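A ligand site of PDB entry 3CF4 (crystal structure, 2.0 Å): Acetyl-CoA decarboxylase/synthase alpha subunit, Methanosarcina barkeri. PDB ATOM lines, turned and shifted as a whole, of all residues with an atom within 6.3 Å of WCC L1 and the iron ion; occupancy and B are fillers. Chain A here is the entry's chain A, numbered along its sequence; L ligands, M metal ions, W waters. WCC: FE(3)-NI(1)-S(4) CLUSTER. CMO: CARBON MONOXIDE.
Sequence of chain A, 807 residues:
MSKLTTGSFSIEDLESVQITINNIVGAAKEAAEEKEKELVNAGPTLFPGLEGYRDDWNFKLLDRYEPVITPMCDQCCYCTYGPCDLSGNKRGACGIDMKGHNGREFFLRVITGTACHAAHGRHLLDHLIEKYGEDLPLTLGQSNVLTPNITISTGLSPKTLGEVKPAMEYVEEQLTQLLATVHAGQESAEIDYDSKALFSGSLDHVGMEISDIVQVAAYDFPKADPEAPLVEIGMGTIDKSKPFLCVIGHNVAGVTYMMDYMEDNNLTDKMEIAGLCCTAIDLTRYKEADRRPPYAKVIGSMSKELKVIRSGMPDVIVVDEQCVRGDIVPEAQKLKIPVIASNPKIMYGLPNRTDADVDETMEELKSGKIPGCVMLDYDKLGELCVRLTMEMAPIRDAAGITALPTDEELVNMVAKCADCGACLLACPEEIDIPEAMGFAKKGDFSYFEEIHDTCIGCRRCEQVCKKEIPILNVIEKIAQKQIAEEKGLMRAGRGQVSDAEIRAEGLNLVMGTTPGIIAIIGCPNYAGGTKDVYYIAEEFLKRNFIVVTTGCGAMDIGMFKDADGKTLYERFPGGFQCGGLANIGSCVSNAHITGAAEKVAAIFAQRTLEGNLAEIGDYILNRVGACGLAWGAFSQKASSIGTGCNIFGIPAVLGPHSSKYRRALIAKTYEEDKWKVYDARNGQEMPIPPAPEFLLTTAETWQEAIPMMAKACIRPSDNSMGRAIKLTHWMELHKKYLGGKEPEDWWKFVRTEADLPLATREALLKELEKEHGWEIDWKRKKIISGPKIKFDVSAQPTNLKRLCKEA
S3 of WCC L1 lies close to N of Cys 278 (3.7 Å).
A sulfur (S4) of WCC L1 sits close to the side-chain hydroxyl (OG) of Ser 635 (3.3 Å).
The backbone NH (N) of Cys 552 sits close to a sulfur (S1) of WCC L1, 3.7 Å away.
A ring nitrogen (NE2) of His 117 lies close to an oxygen (O) of CMO L2, at 3.3 Å.
A sulfur (S4) of WCC L1 lies close to the side-chain amino group (NZ) of Lys 637 (3.6 Å).
SG of Cys 323 binds FE1 of WCC L1 (2.4 Å).
N of Cys 523 sits close to S1 of WCC L1, at 3.2 Å.
SG of Cys 523 binds FE3 of WCC L1.
A nickel atom (NI) of WCC L1 is bound by the side-chain sulfur of Cys 587 (2.3 Å).
The side-chain sulfur of Cys 552 is bound to an iron atom (FE4) of WCC L1.
O of CMO L2 binds NI of WCC L1.
The side-chain amide nitrogen (ND2) of Asn 590 sits at hydrogen-bond distance from the backbone carbonyl oxygen (O) of Cys 587, at 3.0 Å.
SG of Cys 323 sits close to NZ of Lys 637, at 3.5 Å.
The backbone carbonyl oxygen (O) of Cys 323 sits at hydrogen-bond distance from the side-chain sulfur (SG) of Cys 277 (3.8 Å).
NZ of Lys 637 lies within hydrogen-bond range of OE1 of Gln 322.
The backbone carbonyl oxygen (O) of Gln 322 lies within hydrogen-bond range of a ring nitrogen (ND1) of His 250 (3.0 Å).
The backbone NH (N) of Gly 553 is in hydrogen-bond range of the backbone carbonyl oxygen (O) of Gly 522.
N of Cys 587 lies close to SG of Cys 278 (3.2 Å).
The side-chain hydroxyl of Ser 635 sits close to the backbone NH of Lys 637 (3.4 Å).
The backbone carbonyl oxygen (O) of Gly 522 sits close to a sulfur (S1) of WCC L1, 3.4 Å away.
Merely in contact with WCC L1: Pro 524 (3.6 Å), Phe 634 (3.6 Å) and Cys 277 (3.7 Å).
Hydrophobic or aromatic side chains that line WCC L1: His 250, Pro 524 and Phe 634.
Within 4 Å of WCC L1: His 250, Cys 277, Cys 278, Cys 323, Gly 522, Cys 523, Pro 524, Cys 552, Cys 587, Phe 634, Ser 635 and Lys 637.
The nearest printed residue that does not touch WCC L1 is Met 302 (4.04 Å).
NZ of Lys 637 touches the iron ion (3.9 Å).
Within 4 Å of the iron ion: His 250, Cys 278, Cys 587 and Lys 637.
Along chain A the residues within 4 Å of the iron ion span positions 250 to 637.
The nearest printed residue that does not touch the iron ion is Cys 323 (4.8 Å).
The iron ion is bound by a ring nitrogen (NE2) of His 250 (2.0 Å).
Water W1 binds the iron ion, 2.1 Å away.
The iron ion is bound by a sulfur (S3) of WCC L1 (2.3 Å).
The iron ion is bound by SG of Cys 278, 2.4 Å away.
Slightly farther from the iron ion lies the side-chain sulfur (SG) of Cys 587 (2.9 Å).
Water W2 bridges N of Cys 278 and N of Cys 552.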
ATOM      1  N   HIS A 117       5.421   6.276  23.350  1.00  0.00           N
ATOM      2  CA  HIS A 117       6.009   6.907  24.514  1.00  0.00           C
ATOM      3  C   HIS A 117       5.725   8.405  24.479  1.00  0.00           C
ATOM      4  O   HIS A 117       5.490   9.010  25.540  1.00  0.00           O
ATOM      5  CB  HIS A 117       7.513   6.654  24.542  1.00  0.00           C
ATOM      6  CG  HIS A 117       7.870   5.209  24.713  1.00  0.00           C
ATOM      7  ND1 HIS A 117       8.787   4.574  23.904  1.00  0.00           N
ATOM      8  CD2 HIS A 117       7.440   4.279  25.600  1.00  0.00           C
ATOM      9  CE1 HIS A 117       8.897   3.306  24.284  1.00  0.00           C
ATOM     10  NE2 HIS A 117       8.094   3.110  25.308  1.00  0.00           N
ATOM     11  N   GLY A 249      -2.267  -1.490  31.893  1.00  0.00           N
ATOM     12  CA  GLY A 249      -1.961  -0.373  31.026  1.00  0.00           C
ATOM     13  C   GLY A 249      -0.617   0.277  31.245  1.00  0.00           C
ATOM     14  O   GLY A 249       0.332  -0.350  31.729  1.00  0.00           O
ATOM     15  N   HIS A 250      -0.577   1.563  30.900  1.00  0.00           N
ATOM     16  CA  HIS A 250       0.650   2.355  30.996  1.00  0.00           C
ATOM     17  C   HIS A 250       0.560   3.699  31.711  1.00  0.00           C
ATOM     18  O   HIS A 250       1.419   4.015  32.530  1.00  0.00           O
ATOM     19  CB  HIS A 250       1.207   2.562  29.595  1.00  0.00           C
ATOM     20  CG  HIS A 250       1.968   1.388  29.104  1.00  0.00           C
ATOM     21  ND1 HIS A 250       1.379   0.243  28.592  1.00  0.00           N
ATOM     22  CD2 HIS A 250       3.287   1.078  29.239  1.00  0.00           C
ATOM     23  CE1 HIS A 250       2.345  -0.682  28.464  1.00  0.00           C
ATOM     24  NE2 HIS A 250       3.500  -0.202  28.848  1.00  0.00           N
ATOM     25  N   CYS A 277       1.685  -4.996  33.376  1.00  0.00           N
ATOM     26  CA  CYS A 277       2.465  -4.116  32.496  1.00  0.00           C
ATOM     27  C   CYS A 277       2.945  -2.876  33.254  1.00  0.00           C
ATOM     28  O   CYS A 277       2.818  -2.803  34.477  1.00  0.00           O
ATOM     29  CB  CYS A 277       1.645  -3.721  31.265  1.00  0.00           C
ATOM     30  SG  CYS A 277       1.045  -5.147  30.331  1.00  0.00           S
ATOM     31  N   CYS A 278       3.480  -1.909  32.536  1.00  0.00           N
ATOM     32  CA  CYS A 278       4.043  -0.717  33.167  1.00  0.00           C
ATOM     33  C   CYS A 278       3.251   0.019  34.246  1.00  0.00           C
ATOM     34  O   CYS A 278       3.838   0.504  35.222  1.00  0.00           O
ATOM     35  CB  CYS A 278       4.467   0.278  32.089  1.00  0.00           C
ATOM     36  SG  CYS A 278       5.948  -0.239  31.172  1.00  0.00           S
ATOM     37  N   THR A 279       1.938   0.097  34.088  1.00  0.00           N
ATOM     38  CA  THR A 279       1.129   0.802  35.066  1.00  0.00           C
ATOM     39  C   THR A 279       1.315   0.197  36.450  1.00  0.00           C
ATOM     40  O   THR A 279       1.141   0.863  37.461  1.00  0.00           O
ATOM     41  CB  THR A 279      -0.346   0.797  34.679  1.00  0.00           C
ATOM     42  OG1 THR A 279      -1.065   1.670  35.563  1.00  0.00           O
ATOM     43  CG2 THR A 279      -0.927  -0.600  34.772  1.00  0.00           C
ATOM     44  N   SER A 301       3.830  -9.253  34.037  1.00  0.00           N
ATOM     45  CA  SER A 301       3.985  -8.779  32.670  1.00  0.00           C
ATOM     46  C   SER A 301       2.733  -8.958  31.854  1.00  0.00           C
ATOM     47  O   SER A 301       1.706  -9.453  32.335  1.00  0.00           O
ATOM     48  CB  SER A 301       5.131  -9.517  31.978  1.00  0.00           C
ATOM     49  OG  SER A 301       4.772 -10.879  31.766  1.00  0.00           O
ATOM     50  N   MET A 302       2.815  -8.556  30.586  1.00  0.00           N
ATOM     51  CA  MET A 302       1.699  -8.673  29.682  1.00  0.00           C
ATOM     52  C   MET A 302       1.251 -10.124  29.559  1.00  0.00           C
ATOM     53  O   MET A 302       0.085 -10.403  29.316  1.00  0.00           O
ATOM     54  CB  MET A 302       2.077  -8.117  28.318  1.00  0.00           C
ATOM     55  CG  MET A 302       1.038  -8.363  27.250  1.00  0.00           C
ATOM     56  SD  MET A 302       1.559  -7.763  25.667  1.00  0.00           S
ATOM     57  CE  MET A 302       0.040  -7.926  24.737  1.00  0.00           C
ATOM     58  N   GLN A 322      -1.878   0.687  25.619  1.00  0.00           N
ATOM     59  CA  GLN A 322      -0.648  -0.019  25.256  1.00  0.00           C
ATOM     60  C   GLN A 322      -0.463  -1.372  25.912  1.00  0.00           C
ATOM     61  O   GLN A 322      -0.539  -1.490  27.134  1.00  0.00           O
ATOM     62  CB  GLN A 322       0.566   0.869  25.556  1.00  0.00           C
ATOM     63  CG  GLN A 322       0.621   2.114  24.689  1.00  0.00           C
ATOM     64  CD  GLN A 322       1.619   3.126  25.187  1.00  0.00           C
ATOM     65  OE1 GLN A 322       2.630   2.776  25.802  1.00  0.00           O
ATOM     66  NE2 GLN A 322       1.344   4.401  24.914  1.00  0.00           N
ATOM     67  N   CYS A 323      -0.227  -2.379  25.084  1.00  0.00           N
ATOM     68  CA  CYS A 323       0.015  -3.742  25.556  1.00  0.00           C
ATOM     69  C   CYS A 323      -1.165  -4.310  26.321  1.00  0.00           C
ATOM     70  O   CYS A 323      -1.002  -5.185  27.185  1.00  0.00           O
ATOM     71  CB  CYS A 323       1.271  -3.748  26.416  1.00  0.00           C
ATOM     72  SG  CYS A 323       2.693  -2.993  25.564  1.00  0.00           S
ATOM     73  N   ILE A 521      15.904  -5.306  29.821  1.00  0.00           N
ATOM     74  CA  ILE A 521      14.637  -4.611  29.653  1.00  0.00           C
ATOM     75  C   ILE A 521      13.684  -5.298  28.697  1.00  0.00           C
ATOM     76  O   ILE A 521      13.983  -6.362  28.156  1.00  0.00           O
ATOM     77  CB  ILE A 521      14.920  -3.222  29.089  1.00  0.00           C
ATOM     78  CG1 ILE A 521      15.516  -3.377  27.681  1.00  0.00           C
ATOM     79  CG2 ILE A 521      15.897  -2.494  29.973  1.00  0.00           C
ATOM     80  CD1 ILE A 521      15.712  -2.088  26.913  1.00  0.00           C
ATOM     81  N   GLY A 522      12.542  -4.669  28.485  1.00  0.00           N
ATOM     82  CA  GLY A 522      11.613  -5.208  27.512  1.00  0.00           C
ATOM     83  C   GLY A 522      10.566  -6.246  27.859  1.00  0.00           C
ATOM     84  O   GLY A 522      10.484  -6.750  28.988  1.00  0.00           O
ATOM     85  N   CYS A 523       9.809  -6.577  26.813  1.00  0.00           N
ATOM     86  CA  CYS A 523       8.662  -7.479  26.804  1.00  0.00           C
ATOM     87  C   CYS A 523       8.849  -8.925  27.224  1.00  0.00           C
ATOM     88  O   CYS A 523       9.973  -9.414  27.324  1.00  0.00           O
ATOM     89  CB  CYS A 523       8.041  -7.425  25.393  1.00  0.00           C
ATOM     90  SG  CYS A 523       8.084  -5.749  24.645  1.00  0.00           S
ATOM     91  N   PRO A 524       7.737  -9.642  27.480  1.00  0.00           N
ATOM     92  CA  PRO A 524       7.808 -11.045  27.896  1.00  0.00           C
ATOM     93  C   PRO A 524       7.560 -12.100  26.814  1.00  0.00           C
ATOM     94  O   PRO A 524       7.129 -13.209  27.124  1.00  0.00           O
ATOM     95  CB  PRO A 524       6.760 -11.121  29.012  1.00  0.00           C
ATOM     96  CG  PRO A 524       5.665 -10.282  28.424  1.00  0.00           C
ATOM     97  CD  PRO A 524       6.403  -9.090  27.785  1.00  0.00           C
ATOM     98  N   THR A 550      14.198  -2.721  33.647  1.00  0.00           N
ATOM     99  CA  THR A 550      12.959  -1.961  33.574  1.00  0.00           C
ATOM    100  C   THR A 550      11.842  -2.851  33.044  1.00  0.00           C
ATOM    101  O   THR A 550      12.077  -3.976  32.600  1.00  0.00           O
ATOM    102  CB  THR A 550      13.074  -0.766  32.614  1.00  0.00           C
ATOM    103  OG1 THR A 550      13.327  -1.255  31.294  1.00  0.00           O
ATOM    104  CG2 THR A 550      14.193   0.194  33.036  1.00  0.00           C
ATOM    105  N   GLY A 551      10.623  -2.337  33.098  1.00  0.00           N
ATOM    106  CA  GLY A 551       9.469  -3.046  32.565  1.00  0.00           C
ATOM    107  C   GLY A 551       9.253  -4.501  32.922  1.00  0.00           C
ATOM    108  O   GLY A 551       9.601  -4.952  34.013  1.00  0.00           O
ATOM    109  N   CYS A 552       8.669  -5.249  31.994  1.00  0.00           N
ATOM    110  CA  CYS A 552       8.383  -6.648  32.242  1.00  0.00           C
ATOM    111  C   CYS A 552       9.651  -7.412  32.660  1.00  0.00           C
ATOM    112  O   CYS A 552       9.577  -8.362  33.437  1.00  0.00           O
ATOM    113  CB  CYS A 552       7.706  -7.243  30.988  1.00  0.00           C
ATOM    114  SG  CYS A 552       6.054  -6.488  30.650  1.00  0.00           S
ATOM    115  N   GLY A 553      10.807  -6.989  32.171  1.00  0.00           N
ATOM    116  CA  GLY A 553      12.031  -7.645  32.553  1.00  0.00           C
ATOM    117  C   GLY A 553      12.300  -7.472  34.050  1.00  0.00           C
ATOM    118  O   GLY A 553      12.690  -8.420  34.747  1.00  0.00           O
ATOM    119  N   SER A 586       9.432   1.977  34.914  1.00  0.00           N
ATOM    120  CA  SER A 586       8.610   1.422  33.838  1.00  0.00           C
ATOM    121  C   SER A 586       9.384   1.586  32.524  1.00  0.00           C
ATOM    122  O   SER A 586      10.479   2.129  32.508  1.00  0.00           O
ATOM    123  CB  SER A 586       7.251   2.141  33.778  1.00  0.00           C
ATOM    124  OG  SER A 586       7.424   3.546  33.706  1.00  0.00           O
ATOM    125  N   CYS A 587       8.835   1.094  31.410  1.00  0.00           N
ATOM    126  CA  CYS A 587       9.468   1.213  30.096  1.00  0.00           C
ATOM    127  C   CYS A 587       9.889   2.632  29.712  1.00  0.00           C
ATOM    128  O   CYS A 587      10.889   2.826  29.000  1.00  0.00           O
ATOM    129  CB  CYS A 587       8.542   0.633  29.043  1.00  0.00           C
ATOM    130  SG  CYS A 587       8.263  -1.134  29.324  1.00  0.00           S
ATOM    131  N   VAL A 588       9.152   3.654  30.146  1.00  0.00           N
ATOM    132  CA  VAL A 588       9.565   5.019  29.783  1.00  0.00           C
ATOM    133  C   VAL A 588      10.854   5.366  30.539  1.00  0.00           C
ATOM    134  O   VAL A 588      11.592   6.252  30.115  1.00  0.00           O
ATOM    135  CB  VAL A 588       8.482   6.114  30.089  1.00  0.00           C
ATOM    136  CG1 VAL A 588       7.351   6.043  29.063  1.00  0.00           C
ATOM    137  CG2 VAL A 588       7.945   5.975  31.507  1.00  0.00           C
ATOM    138  N   ASN A 590      13.432   3.700  30.579  1.00  0.00           N
ATOM    139  CA  ASN A 590      14.592   3.257  29.840  1.00  0.00           C
ATOM    140  C   ASN A 590      15.401   4.497  29.450  1.00  0.00           C
ATOM    141  O   ASN A 590      16.601   4.410  29.231  1.00  0.00           O
ATOM    142  CB  ASN A 590      14.187   2.475  28.593  1.00  0.00           C
ATOM    143  CG  ASN A 590      13.826   1.027  28.911  1.00  0.00           C
ATOM    144  OD1 ASN A 590      14.564   0.335  29.619  1.00  0.00           O
ATOM    145  ND2 ASN A 590      12.699   0.563  28.366  1.00  0.00           N
ATOM    146  N   GLY A 632      12.721 -10.807  25.538  1.00  0.00           N
ATOM    147  CA  GLY A 632      11.371 -11.139  25.100  1.00  0.00           C
ATOM    148  C   GLY A 632      10.700 -10.003  24.347  1.00  0.00           C
ATOM    149  O   GLY A 632       9.477  -9.831  24.429  1.00  0.00           O
ATOM    150  N   PHE A 634       8.775  -7.748  21.974  1.00  0.00           N
ATOM    151  CA  PHE A 634       7.615  -8.029  21.124  1.00  0.00           C
ATOM    152  C   PHE A 634       7.024  -6.772  20.505  1.00  0.00           C
ATOM    153  O   PHE A 634       6.634  -6.766  19.337  1.00  0.00           O
ATOM    154  CB  PHE A 634       6.521  -8.720  21.977  1.00  0.00           C
ATOM    155  CG  PHE A 634       5.276  -7.876  22.182  1.00  0.00           C
ATOM    156  CD1 PHE A 634       4.323  -7.748  21.173  1.00  0.00           C
ATOM    157  CD2 PHE A 634       5.058  -7.217  23.387  1.00  0.00           C
ATOM    158  CE1 PHE A 634       3.180  -6.967  21.355  1.00  0.00           C
ATOM    159  CE2 PHE A 634       3.914  -6.423  23.590  1.00  0.00           C
ATOM    160  CZ  PHE A 634       2.976  -6.300  22.566  1.00  0.00           C
ATOM    161  N   SER A 635       6.937  -5.721  21.309  1.00  0.00           N
ATOM    162  CA  SER A 635       6.328  -4.450  20.928  1.00  0.00           C
ATOM    163  C   SER A 635       7.089  -3.539  19.981  1.00  0.00           C
ATOM    164  O   SER A 635       8.306  -3.630  19.818  1.00  0.00           O
ATOM    165  CB  SER A 635       6.020  -3.650  22.200  1.00  0.00           C
ATOM    166  OG  SER A 635       7.235  -3.195  22.776  1.00  0.00           O
ATOM    167  N   LYS A 637       7.381  -0.543  20.581  1.00  0.00           N
ATOM    168  CA  LYS A 637       8.139   0.257  21.538  1.00  0.00           C
ATOM    169  C   LYS A 637       9.524  -0.334  21.798  1.00  0.00           C
ATOM    170  O   LYS A 637      10.505   0.404  21.955  1.00  0.00           O
ATOM    171  CB  LYS A 637       7.374   0.374  22.861  1.00  0.00           C
ATOM    172  CG  LYS A 637       6.288   1.464  22.837  1.00  0.00           C
ATOM    173  CD  LYS A 637       5.497   1.527  24.141  1.00  0.00           C
ATOM    174  CE  LYS A 637       4.536   0.366  24.235  1.00  0.00           C
ATOM    175  NZ  LYS A 637       3.895   0.267  25.580  1.00  0.00           N
ATOM    176  N   ALA A 638       9.627  -1.662  21.824  1.00  0.00           N
ATOM    177  CA  ALA A 638      10.934  -2.269  22.059  1.00  0.00           C
ATOM    178  C   ALA A 638      11.888  -1.968  20.899  1.00  0.00           C
ATOM    179  O   ALA A 638      13.081  -1.732  21.111  1.00  0.00           O
ATOM    180  CB  ALA A 638      10.794  -3.785  22.274  1.00  0.00           C
ATOM    181  N   ILE A 641      13.095   1.659  21.342  1.00  0.00           N
ATOM    182  CA  ILE A 641      14.023   1.776  22.471  1.00  0.00           C
ATOM    183  C   ILE A 641      15.402   1.238  22.077  1.00  0.00           C
ATOM    184  O   ILE A 641      16.423   1.906  22.263  1.00  0.00           O
ATOM    185  CB  ILE A 641      13.525   1.004  23.700  1.00  0.00           C
ATOM    186  CG1 ILE A 641      12.290   1.692  24.273  1.00  0.00           C
ATOM    187  CG2 ILE A 641      14.622   0.991  24.771  1.00  0.00           C
ATOM    188  CD1 ILE A 641      11.505   0.804  25.196  1.00  0.00           C
HETATM  189 NI   WCC L   1       7.787  -2.229  27.393  1.00  0.00          NI
HETATM  190 FE1  WCC L   1       4.562  -3.578  26.901  1.00  0.00          FE
HETATM  191 FE3  WCC L   1       7.025  -4.609  26.382  1.00  0.00          FE
HETATM  192 FE4  WCC L   1       6.044  -4.941  28.880  1.00  0.00          FE
HETATM  193  S1  WCC L   1       8.218  -4.268  28.407  1.00  0.00           S
HETATM  194  S2  WCC L   1       5.119  -5.837  26.947  1.00  0.00           S
HETATM  195  S3  WCC L   1       4.630  -3.136  29.200  1.00  0.00           S
HETATM  196  S4  WCC L   1       6.241  -2.466  25.803  1.00  0.00           S
HETATM  197  C   CMO L   2       9.111  -1.123  26.363  1.00  0.00           C
HETATM  198  O   CMO L   2       8.492  -0.109  26.116  1.00  0.00           O
HETATM  199 FE    FE M   1       5.378  -0.985  29.017  1.00  0.00          FE
HETATM  200  O   HOH W   1       5.976   0.046  27.246  1.00  0.00           O
HETATM  201  O   HOH W   2       5.956  -3.591  32.214  1.00  0.00           O
